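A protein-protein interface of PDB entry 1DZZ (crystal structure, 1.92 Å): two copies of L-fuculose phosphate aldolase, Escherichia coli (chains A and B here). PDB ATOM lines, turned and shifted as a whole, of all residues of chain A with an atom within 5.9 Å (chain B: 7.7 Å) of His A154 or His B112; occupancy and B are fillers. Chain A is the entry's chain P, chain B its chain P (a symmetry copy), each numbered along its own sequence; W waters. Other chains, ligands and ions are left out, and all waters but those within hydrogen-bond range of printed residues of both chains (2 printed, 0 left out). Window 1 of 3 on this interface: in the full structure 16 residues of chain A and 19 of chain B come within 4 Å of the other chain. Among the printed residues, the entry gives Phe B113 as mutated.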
ATOM      1  N   HIS A  94      27.552   8.021  20.416  1.00  0.00           N
ATOM      2  CA  HIS A  94      27.242   6.881  19.574  1.00  0.00           C
ATOM      3  C   HIS A  94      28.581   6.404  18.981  1.00  0.00           C
ATOM      4  O   HIS A  94      28.688   6.181  17.778  1.00  0.00           O
ATOM      5  CB  HIS A  94      26.221   7.223  18.495  1.00  0.00           C
ATOM      6  CG  HIS A  94      24.885   7.739  18.942  1.00  0.00           C
ATOM      7  ND1 HIS A  94      23.960   8.175  18.018  1.00  0.00           N
ATOM      8  CD2 HIS A  94      24.269   7.895  20.135  1.00  0.00           C
ATOM      9  CE1 HIS A  94      22.861   8.617  18.617  1.00  0.00           C
ATOM     10  NE2 HIS A  94      23.038   8.452  19.919  1.00  0.00           N
ATOM     11  N   THR A  99      28.797   1.094  19.852  1.00  0.00           N
ATOM     12  CA  THR A  99      27.511   0.949  19.160  1.00  0.00           C
ATOM     13  C   THR A  99      27.442  -0.366  18.410  1.00  0.00           C
ATOM     14  O   THR A  99      26.382  -0.992  18.462  1.00  0.00           O
ATOM     15  CB  THR A  99      27.260   2.147  18.230  1.00  0.00           C
ATOM     16  OG1 THR A  99      27.333   3.374  18.988  1.00  0.00           O
ATOM     17  CG2 THR A  99      25.896   1.996  17.568  1.00  0.00           C
ATOM     18  N   SER A 102      26.699  -2.927  20.847  1.00  0.00           N
ATOM     19  CA  SER A 102      25.317  -2.775  21.310  1.00  0.00           C
ATOM     20  C   SER A 102      24.315  -3.339  20.302  1.00  0.00           C
ATOM     21  O   SER A 102      23.202  -3.713  20.684  1.00  0.00           O
ATOM     22  CB  SER A 102      24.978  -1.332  21.633  1.00  0.00           C
ATOM     23  OG  SER A 102      24.533  -0.635  20.477  1.00  0.00           O
ATOM     24  N   ILE A 103      24.718  -3.412  19.039  1.00  0.00           N
ATOM     25  CA  ILE A 103      23.887  -3.991  17.986  1.00  0.00           C
ATOM     26  C   ILE A 103      23.812  -5.497  18.155  1.00  0.00           C
ATOM     27  O   ILE A 103      22.804  -6.187  17.898  1.00  0.00           O
ATOM     28  CB  ILE A 103      24.437  -3.534  16.617  1.00  0.00           C
ATOM     29  CG1 ILE A 103      24.027  -2.076  16.380  1.00  0.00           C
ATOM     30  CG2 ILE A 103      23.952  -4.420  15.491  1.00  0.00           C
ATOM     31  CD1 ILE A 103      24.638  -1.417  15.154  1.00  0.00           C
ATOM     32  N   CYS A 125      24.841  -4.163  28.680  1.00  0.00           N
ATOM     33  CA  CYS A 125      24.132  -3.672  27.501  1.00  0.00           C
ATOM     34  C   CYS A 125      22.639  -3.668  27.862  1.00  0.00           C
ATOM     35  O   CYS A 125      22.079  -4.760  27.985  1.00  0.00           O
ATOM     36  CB  CYS A 125      24.373  -4.535  26.258  1.00  0.00           C
ATOM     37  SG  CYS A 125      23.566  -3.802  24.790  1.00  0.00           S
ATOM     38  N   TYR A 128      16.966  -2.271  24.231  1.00  0.00           N
ATOM     39  CA  TYR A 128      16.448  -1.213  23.411  1.00  0.00           C
ATOM     40  C   TYR A 128      15.119  -0.642  23.882  1.00  0.00           C
ATOM     41  O   TYR A 128      14.203  -1.380  24.206  1.00  0.00           O
ATOM     42  CB  TYR A 128      16.292  -1.685  21.929  1.00  0.00           C
ATOM     43  CG  TYR A 128      15.733  -0.563  21.062  1.00  0.00           C
ATOM     44  CD1 TYR A 128      16.564   0.425  20.581  1.00  0.00           C
ATOM     45  CD2 TYR A 128      14.378  -0.460  20.785  1.00  0.00           C
ATOM     46  CE1 TYR A 128      16.088   1.487  19.831  1.00  0.00           C
ATOM     47  CE2 TYR A 128      13.893   0.597  20.036  1.00  0.00           C
ATOM     48  CZ  TYR A 128      14.732   1.556  19.543  1.00  0.00           C
ATOM     49  OH  TYR A 128      14.290   2.611  18.795  1.00  0.00           O
ATOM     50  N   LEU A 152      23.851   0.734  25.263  1.00  0.00           N
ATOM     51  CA  LEU A 152      22.423   0.853  25.016  1.00  0.00           C
ATOM     52  C   LEU A 152      22.173   0.088  23.703  1.00  0.00           C
ATOM     53  O   LEU A 152      22.755   0.516  22.703  1.00  0.00           O
ATOM     54  CB  LEU A 152      22.020   2.316  24.797  1.00  0.00           C
ATOM     55  CG  LEU A 152      22.005   3.187  26.068  1.00  0.00           C
ATOM     56  CD1 LEU A 152      23.404   3.657  26.407  1.00  0.00           C
ATOM     57  CD2 LEU A 152      21.135   4.409  25.869  1.00  0.00           C
ATOM     58  N   GLN A 153      21.400  -0.980  23.750  1.00  0.00           N
ATOM     59  CA  GLN A 153      21.170  -1.774  22.540  1.00  0.00           C
ATOM     60  C   GLN A 153      20.673  -0.967  21.365  1.00  0.00           C
ATOM     61  O   GLN A 153      19.766  -0.173  21.448  1.00  0.00           O
ATOM     62  CB  GLN A 153      20.254  -2.967  22.832  1.00  0.00           C
ATOM     63  CG  GLN A 153      19.898  -3.791  21.612  1.00  0.00           C
ATOM     64  CD  GLN A 153      18.809  -4.820  21.917  1.00  0.00           C
ATOM     65  OE1 GLN A 153      18.674  -5.779  21.145  1.00  0.00           O
ATOM     66  NE2 GLN A 153      18.102  -4.695  23.022  1.00  0.00           N
ATOM     67  N   HIS A 154      21.294  -1.155  20.200  1.00  0.00           N
ATOM     68  CA  HIS A 154      21.003  -0.470  18.960  1.00  0.00           C
ATOM     69  C   HIS A 154      21.140   1.046  19.081  1.00  0.00           C
ATOM     70  O   HIS A 154      20.423   1.775  18.377  1.00  0.00           O
ATOM     71  CB  HIS A 154      19.560  -0.719  18.456  1.00  0.00           C
ATOM     72  CG  HIS A 154      19.439  -2.087  17.886  1.00  0.00           C
ATOM     73  ND1 HIS A 154      20.084  -2.492  16.737  1.00  0.00           N
ATOM     74  CD2 HIS A 154      18.754  -3.164  18.364  1.00  0.00           C
ATOM     75  CE1 HIS A 154      19.795  -3.776  16.529  1.00  0.00           C
ATOM     76  NE2 HIS A 154      18.997  -4.196  17.494  1.00  0.00           N
ATOM     77  N   HIS A 155      22.118   1.489  19.900  1.00  0.00           N
ATOM     78  CA  HIS A 155      22.108   2.938  20.125  1.00  0.00           C
ATOM     79  C   HIS A 155      23.483   3.514  20.399  1.00  0.00           C
ATOM     80  O   HIS A 155      23.950   4.336  19.599  1.00  0.00           O
ATOM     81  CB  HIS A 155      21.106   3.133  21.281  1.00  0.00           C
ATOM     82  CG  HIS A 155      20.858   4.566  21.623  1.00  0.00           C
ATOM     83  ND1 HIS A 155      19.645   4.989  22.087  1.00  0.00           N
ATOM     84  CD2 HIS A 155      21.628   5.673  21.538  1.00  0.00           C
ATOM     85  CE1 HIS A 155      19.672   6.306  22.301  1.00  0.00           C
ATOM     86  NE2 HIS A 155      20.881   6.736  21.963  1.00  0.00           N
ATOM     87  N   GLY A 156      24.105   3.145  21.514  1.00  0.00           N
ATOM     88  CA  GLY A 156      25.388   3.763  21.858  1.00  0.00           C
ATOM     89  C   GLY A 156      25.808   3.499  23.300  1.00  0.00           C
ATOM     90  O   GLY A 156      25.673   2.403  23.842  1.00  0.00           O
ATOM     91  N   ILE B 108      21.735  -1.363   3.361  1.00  0.00           N
ATOM     92  CA  ILE B 108      21.953  -1.371   4.812  1.00  0.00           C
ATOM     93  C   ILE B 108      20.574  -1.435   5.482  1.00  0.00           C
ATOM     94  O   ILE B 108      19.771  -0.537   5.232  1.00  0.00           O
ATOM     95  CB  ILE B 108      22.612  -0.065   5.240  1.00  0.00           C
ATOM     96  CG1 ILE B 108      23.892   0.074   4.416  1.00  0.00           C
ATOM     97  CG2 ILE B 108      22.874  -0.022   6.750  1.00  0.00           C
ATOM     98  CD1 ILE B 108      24.545   1.416   4.523  1.00  0.00           C
ATOM     99  N   PRO B 109      20.298  -2.468   6.256  1.00  0.00           N
ATOM    100  CA  PRO B 109      19.031  -2.600   6.964  1.00  0.00           C
ATOM    101  C   PRO B 109      19.047  -1.778   8.237  1.00  0.00           C
ATOM    102  O   PRO B 109      20.035  -1.109   8.580  1.00  0.00           O
ATOM    103  CB  PRO B 109      18.966  -4.109   7.217  1.00  0.00           C
ATOM    104  CG  PRO B 109      20.388  -4.504   7.426  1.00  0.00           C
ATOM    105  CD  PRO B 109      21.217  -3.581   6.548  1.00  0.00           C
ATOM    106  N   ALA B 110      17.981  -1.809   9.021  1.00  0.00           N
ATOM    107  CA  ALA B 110      17.774  -1.018  10.216  1.00  0.00           C
ATOM    108  C   ALA B 110      18.507  -1.540  11.444  1.00  0.00           C
ATOM    109  O   ALA B 110      17.912  -1.894  12.472  1.00  0.00           O
ATOM    110  CB  ALA B 110      16.272  -0.941  10.492  1.00  0.00           C
ATOM    111  N   ILE B 111      19.833  -1.526  11.407  1.00  0.00           N
ATOM    112  CA  ILE B 111      20.646  -1.965  12.525  1.00  0.00           C
ATOM    113  C   ILE B 111      20.784  -0.926  13.632  1.00  0.00           C
ATOM    114  O   ILE B 111      21.224  -1.212  14.753  1.00  0.00           O
ATOM    115  CB  ILE B 111      22.077  -2.273  12.015  1.00  0.00           C
ATOM    116  CG1 ILE B 111      22.636  -1.044  11.310  1.00  0.00           C
ATOM    117  CG2 ILE B 111      21.961  -3.493  11.125  1.00  0.00           C
ATOM    118  CD1 ILE B 111      24.090  -1.097  10.895  1.00  0.00           C
ATOM    119  N   HIS B 112      20.431   0.308  13.342  1.00  0.00           N
ATOM    120  CA  HIS B 112      20.497   1.428  14.266  1.00  0.00           C
ATOM    121  C   HIS B 112      19.360   2.388  13.943  1.00  0.00           C
ATOM    122  O   HIS B 112      18.989   2.550  12.755  1.00  0.00           O
ATOM    123  CB  HIS B 112      21.835   2.151  14.083  1.00  0.00           C
ATOM    124  CG  HIS B 112      22.123   3.120  15.191  1.00  0.00           C
ATOM    125  ND1 HIS B 112      21.566   4.377  15.288  1.00  0.00           N
ATOM    126  CD2 HIS B 112      22.903   2.963  16.289  1.00  0.00           C
ATOM    127  CE1 HIS B 112      21.994   4.967  16.382  1.00  0.00           C
ATOM    128  NE2 HIS B 112      22.831   4.138  16.999  1.00  0.00           N
ATOM    129  N   PHE B 113      18.809   3.079  14.947  1.00  0.00           N
ATOM    130  CA  PHE B 113      17.654   3.940  14.646  1.00  0.00           C
ATOM    131  C   PHE B 113      17.966   5.166  13.818  1.00  0.00           C
ATOM    132  O   PHE B 113      17.052   5.700  13.171  1.00  0.00           O
ATOM    133  CB  PHE B 113      16.873   4.324  15.903  1.00  0.00           C
ATOM    134  CG  PHE B 113      17.653   5.260  16.783  1.00  0.00           C
ATOM    135  CD1 PHE B 113      17.612   6.618  16.592  1.00  0.00           C
ATOM    136  CD2 PHE B 113      18.397   4.726  17.822  1.00  0.00           C
ATOM    137  CE1 PHE B 113      18.329   7.470  17.418  1.00  0.00           C
ATOM    138  CE2 PHE B 113      19.123   5.557  18.668  1.00  0.00           C
ATOM    139  CZ  PHE B 113      19.078   6.924  18.445  1.00  0.00           C
ATOM    140  N   MET B 114      19.222   5.576  13.693  1.00  0.00           N
ATOM    141  CA  MET B 114      19.590   6.696  12.856  1.00  0.00           C
ATOM    142  C   MET B 114      19.394   6.401  11.379  1.00  0.00           C
ATOM    143  O   MET B 114      19.422   7.373  10.630  1.00  0.00           O
ATOM    144  CB  MET B 114      21.012   7.201  13.098  1.00  0.00           C
ATOM    145  CG  MET B 114      21.097   7.982  14.412  1.00  0.00           C
ATOM    146  SD  MET B 114      20.093   9.482  14.416  1.00  0.00           S
ATOM    147  CE  MET B 114      20.780  10.326  12.994  1.00  0.00           C
ATOM    148  N   ILE B 115      19.132   5.172  10.961  1.00  0.00           N
ATOM    149  CA  ILE B 115      18.821   4.871   9.585  1.00  0.00           C
ATOM    150  C   ILE B 115      17.629   5.656   9.069  1.00  0.00           C
ATOM    151  O   ILE B 115      17.555   6.015   7.886  1.00  0.00           O
ATOM    152  CB  ILE B 115      18.540   3.368   9.398  1.00  0.00           C
ATOM    153  CG1 ILE B 115      18.529   3.081   7.881  1.00  0.00           C
ATOM    154  CG2 ILE B 115      17.236   2.933   9.990  1.00  0.00           C
ATOM    155  CD1 ILE B 115      19.323   1.861   7.530  1.00  0.00           C
ATOM    156  N   ALA B 116      16.705   6.050   9.940  1.00  0.00           N
ATOM    157  CA  ALA B 116      15.564   6.884   9.635  1.00  0.00           C
ATOM    158  C   ALA B 116      15.911   8.269   9.096  1.00  0.00           C
ATOM    159  O   ALA B 116      15.101   8.874   8.384  1.00  0.00           O
ATOM    160  CB  ALA B 116      14.704   7.020  10.892  1.00  0.00           C
ATOM    161  N   ALA B 117      17.141   8.755   9.274  1.00  0.00           N
ATOM    162  CA  ALA B 117      17.555  10.033   8.743  1.00  0.00           C
ATOM    163  C   ALA B 117      17.495  10.061   7.220  1.00  0.00           C
ATOM    164  O   ALA B 117      17.331  11.133   6.627  1.00  0.00           O
ATOM    165  CB  ALA B 117      18.954  10.421   9.232  1.00  0.00           C
ATOM    166  N   GLY B 120      13.574   6.221   5.629  1.00  0.00           N
ATOM    167  CA  GLY B 120      12.893   4.941   5.749  1.00  0.00           C
ATOM    168  C   GLY B 120      13.616   3.956   6.654  1.00  0.00           C
ATOM    169  O   GLY B 120      14.303   4.359   7.614  1.00  0.00           O
ATOM    170  N   ASN B 121      13.471   2.660   6.387  1.00  0.00           N
ATOM    171  CA  ASN B 121      14.122   1.634   7.204  1.00  0.00           C
ATOM    172  C   ASN B 121      15.355   1.021   6.553  1.00  0.00           C
ATOM    173  O   ASN B 121      15.791  -0.073   6.929  1.00  0.00           O
ATOM    174  CB  ASN B 121      13.106   0.502   7.482  1.00  0.00           C
ATOM    175  CG  ASN B 121      12.711  -0.232   6.203  1.00  0.00           C
ATOM    176  OD1 ASN B 121      13.001   0.191   5.090  1.00  0.00           O
ATOM    177  ND2 ASN B 121      12.059  -1.381   6.363  1.00  0.00           N
ATOM    178  N   GLU B 173      26.719  10.320   8.382  1.00  0.00           N
ATOM    179  CA  GLU B 173      25.919   9.358   9.116  1.00  0.00           C
ATOM    180  C   GLU B 173      25.801   8.020   8.357  1.00  0.00           C
ATOM    181  O   GLU B 173      25.784   6.963   8.990  1.00  0.00           O
ATOM    182  CB  GLU B 173      24.502   9.821   9.412  1.00  0.00           C
ATOM    183  CG  GLU B 173      24.206  10.657  10.624  1.00  0.00           C
ATOM    184  CD  GLU B 173      24.712  10.033  11.920  1.00  0.00           C
ATOM    185  OE1 GLU B 173      24.425   8.856  12.257  1.00  0.00           O
ATOM    186  OE2 GLU B 173      25.467  10.786  12.578  1.00  0.00           O
ATOM    187  N   VAL B 176      28.907   6.059   8.864  1.00  0.00           N
ATOM    188  CA  VAL B 176      28.885   5.390  10.165  1.00  0.00           C
ATOM    189  C   VAL B 176      28.033   4.125  10.201  1.00  0.00           C
ATOM    190  O   VAL B 176      28.427   3.054  10.717  1.00  0.00           O
ATOM    191  CB  VAL B 176      28.496   6.359  11.317  1.00  0.00           C
ATOM    192  CG1 VAL B 176      28.241   5.645  12.644  1.00  0.00           C
ATOM    193  CG2 VAL B 176      29.674   7.318  11.487  1.00  0.00           C
ATOM    194  N   LEU B 177      26.839   4.192   9.630  1.00  0.00           N
ATOM    195  CA  LEU B 177      25.943   3.048   9.493  1.00  0.00           C
ATOM    196  C   LEU B 177      26.607   1.939   8.679  1.00  0.00           C
ATOM    197  O   LEU B 177      26.544   0.789   9.086  1.00  0.00           O
ATOM    198  CB  LEU B 177      24.639   3.481   8.797  1.00  0.00           C
ATOM    199  CG  LEU B 177      23.696   4.331   9.658  1.00  0.00           C
ATOM    200  CD1 LEU B 177      22.528   4.874   8.845  1.00  0.00           C
ATOM    201  CD2 LEU B 177      23.200   3.491  10.843  1.00  0.00           C
ATOM    202  N   LEU B 180      29.216   0.339  10.942  1.00  0.00           N
ATOM    203  CA  LEU B 180      28.505  -0.481  11.909  1.00  0.00           C
ATOM    204  C   LEU B 180      28.079  -1.814  11.298  1.00  0.00           C
ATOM    205  O   LEU B 180      28.279  -2.876  11.885  1.00  0.00           O
ATOM    206  CB  LEU B 180      27.233   0.204  12.455  1.00  0.00           C
ATOM    207  CG  LEU B 180      27.505   1.377  13.406  1.00  0.00           C
ATOM    208  CD1 LEU B 180      26.198   2.066  13.728  1.00  0.00           C
ATOM    209  CD2 LEU B 180      28.221   0.898  14.682  1.00  0.00           C
ATOM    210  N   VAL B 191      22.586  -9.586  10.641  1.00  0.00           N
ATOM    211  CA  VAL B 191      22.741  -8.684  11.793  1.00  0.00           C
ATOM    212  C   VAL B 191      21.369  -8.373  12.375  1.00  0.00           C
ATOM    213  O   VAL B 191      20.425  -8.119  11.646  1.00  0.00           O
ATOM    214  CB  VAL B 191      23.436  -7.355  11.393  1.00  0.00           C
ATOM    215  CG1 VAL B 191      23.556  -6.430  12.615  1.00  0.00           C
ATOM    216  CG2 VAL B 191      24.832  -7.563  10.823  1.00  0.00           C
ATOM    217  N   PRO B 192      21.241  -8.355  13.695  1.00  0.00           N
ATOM    218  CA  PRO B 192      19.978  -8.021  14.342  1.00  0.00           C
ATOM    219  C   PRO B 192      19.498  -6.679  13.825  1.00  0.00           C
ATOM    220  O   PRO B 192      20.341  -5.812  13.625  1.00  0.00           O
ATOM    221  CB  PRO B 192      20.326  -7.937  15.832  1.00  0.00           C
ATOM    222  CG  PRO B 192      21.504  -8.850  15.951  1.00  0.00           C
ATOM    223  CD  PRO B 192      22.294  -8.681  14.667  1.00  0.00           C
ATOM    224  N   VAL B 193      18.218  -6.486  13.589  1.00  0.00           N
ATOM    225  CA  VAL B 193      17.680  -5.223  13.135  1.00  0.00           C
ATOM    226  C   VAL B 193      16.498  -4.773  14.000  1.00  0.00           C
ATOM    227  O   VAL B 193      15.908  -5.592  14.701  1.00  0.00           O
ATOM    228  CB  VAL B 193      17.163  -5.269  11.686  1.00  0.00           C
ATOM    229  CG1 VAL B 193      18.339  -5.501  10.743  1.00  0.00           C
ATOM    230  CG2 VAL B 193      16.072  -6.322  11.507  1.00  0.00           C
ATOM    231  N   LEU B 194      16.151  -3.499  13.892  1.00  0.00           N
ATOM    232  CA  LEU B 194      14.956  -3.002  14.566  1.00  0.00           C
ATOM    233  C   LEU B 194      13.784  -3.317  13.641  1.00  0.00           C
ATOM    234  O   LEU B 194      13.915  -3.245  12.424  1.00  0.00           O
ATOM    235  CB  LEU B 194      15.081  -1.496  14.793  1.00  0.00           C
ATOM    236  CG  LEU B 194      16.162  -1.118  15.823  1.00  0.00           C
ATOM    237  CD1 LEU B 194      16.531   0.352  15.664  1.00  0.00           C
ATOM    238  CD2 LEU B 194      15.722  -1.457  17.229  1.00  0.00           C
ATOM    239  N   SER B 195      12.630  -3.655  14.190  1.00  0.00           N
ATOM    240  CA  SER B 195      11.422  -3.935  13.403  1.00  0.00           C
ATOM    241  C   SER B 195      10.878  -2.699  12.710  1.00  0.00           C
ATOM    242  O   SER B 195      11.104  -1.548  13.103  1.00  0.00           O
ATOM    243  CB  SER B 195      10.357  -4.506  14.368  1.00  0.00           C
ATOM    244  OG  SER B 195       9.853  -3.434  15.172  1.00  0.00           O
ATOM    245  N   ILE B 199      10.905   1.406  13.616  1.00  0.00           N
ATOM    246  CA  ILE B 199      11.373   2.490  12.734  1.00  0.00           C
ATOM    247  C   ILE B 199      10.266   3.503  12.460  1.00  0.00           C
ATOM    248  O   ILE B 199      10.489   4.710  12.431  1.00  0.00           O
ATOM    249  CB  ILE B 199      11.977   1.967  11.419  1.00  0.00           C
ATOM    250  CG1 ILE B 199      13.257   1.180  11.755  1.00  0.00           C
ATOM    251  CG2 ILE B 199      12.252   3.096  10.428  1.00  0.00           C
ATOM    252  CD1 ILE B 199      14.429   2.003  12.246  1.00  0.00           C
ATOM    253  N   VAL B 202      10.225   5.960  15.305  1.00  0.00           N
ATOM    254  CA  VAL B 202      11.374   6.862  15.229  1.00  0.00           C
ATOM    255  C   VAL B 202      11.150   7.881  14.132  1.00  0.00           C
ATOM    256  O   VAL B 202      11.411   9.073  14.349  1.00  0.00           O
ATOM    257  CB  VAL B 202      12.665   6.053  15.040  1.00  0.00           C
ATOM    258  CG1 VAL B 202      13.836   6.969  14.693  1.00  0.00           C
ATOM    259  CG2 VAL B 202      12.945   5.297  16.346  1.00  0.00           C
HETATM  260  O   HOH W   1      16.933  -6.343  17.421  1.00  0.00           O
HETATM  261  O   HOH W   2      24.487   8.291  15.427  1.00  0.00           O
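O of Ile B111 lies within hydrogen-bond range of ND1 of His A154 (2.6 Å). NE2 of His B112 sits at hydrogen-bond distance from O of His A155, 2.8 Å away.
The backbone carbonyl oxygen (O) of Ser A102 lies within hydrogen-bond range of the backbone NH (N) of His A154, at 3.2 Å. The side-chain hydroxyl (OG) of Ser A102 is in hydrogen-bond range of the backbone NH (N) of His A155, 3.3 Å away. N of Met B114 lies within hydrogen-bond range of ND1 of His B112 (3.1 Å). The side-chain hydroxyl (OG) of Ser A102 sits at hydrogen-bond distance from the backbone carbonyl oxygen (O) of Thr A99. The backbone NH (N) of Tyr A128 lies close to the side-chain amide nitrogen (NE2) of Gln A153, 2.9 Å away. The backbone carbonyl oxygen (O) of Ala B110 sits at hydrogen-bond distance from the backbone NH (N) of Leu B194 (2.8 Å).
Thr A99 touches His B112. O of Ile B111 touches CG1 of Ile A103, 3.4 Å away. CG2 of Ile A103 touches CG1 of Val B191, 3.5 Å away. O of Ile A103 touches CG of Pro B192 (3.5 Å). CZ of Tyr A128 touches CD2 of Leu B194, 3.9 Å away. Val B202 touches Tyr A128 (CG2 to OH, 3.9 Å). His A154 touches His B112 (O to CD2, 3.5 Å). His A154 touches Phe B113 (O to CD2, 3.6 Å). CD2 of His A154 touches CD2 of Leu B194 (3.7 Å). His A155 touches Phe B113 (ND1 to CE2, 3.5 Å).
His A154 touches just these residues of chain B: Ile B111 (2.6 Å), His B112 (3.5 Å), Phe B113 (3.6 Å), Pro B192 (3.6 Å) and Leu B194 (3.7 Å). Of the printed residues of chain B, His A155 touches His B112 and Phe B113. Printed residues of chain A within 4 Å of Phe B113: His A154 (3.6 Å) and His A155 (3.5 Å). The nearest residue of chain A that does not touch His B112 is His A94 (4.1 Å).
Of the 11 printed residues of chain A, 5 touch a printed residue of chain B. Of the 23 printed residues of chain B, 8 touch a printed residue of chain A. Hydrophobic or aromatic side chains of chain B within 4 Å of the printed part of chain A: His B112, Phe B113, Leu B180, Val B191, Pro B192, Leu B194 and Val B202. Among the printed residues, 14 pairs touch across the chains. Among the printed residues, no Asp or Glu carboxylate lies within 4 Å of a Lys or Arg side-chain nitrogen of the other chain.
No position is printed for both chains. Of the 14 pairs that touch across the chains among the printed residues, none has its exchanged pair printed and touching as well.
Water W2 bridges a ring nitrogen (ND1) of His A94 (2.6 Å) and the side-chain carboxylate of Glu B173 (3.2 Å). Water W1 bridges a ring nitrogen (NE2) of His A154 (3.0 Å) and the backbone carbonyl oxygen of Val B193 (3.0 Å).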
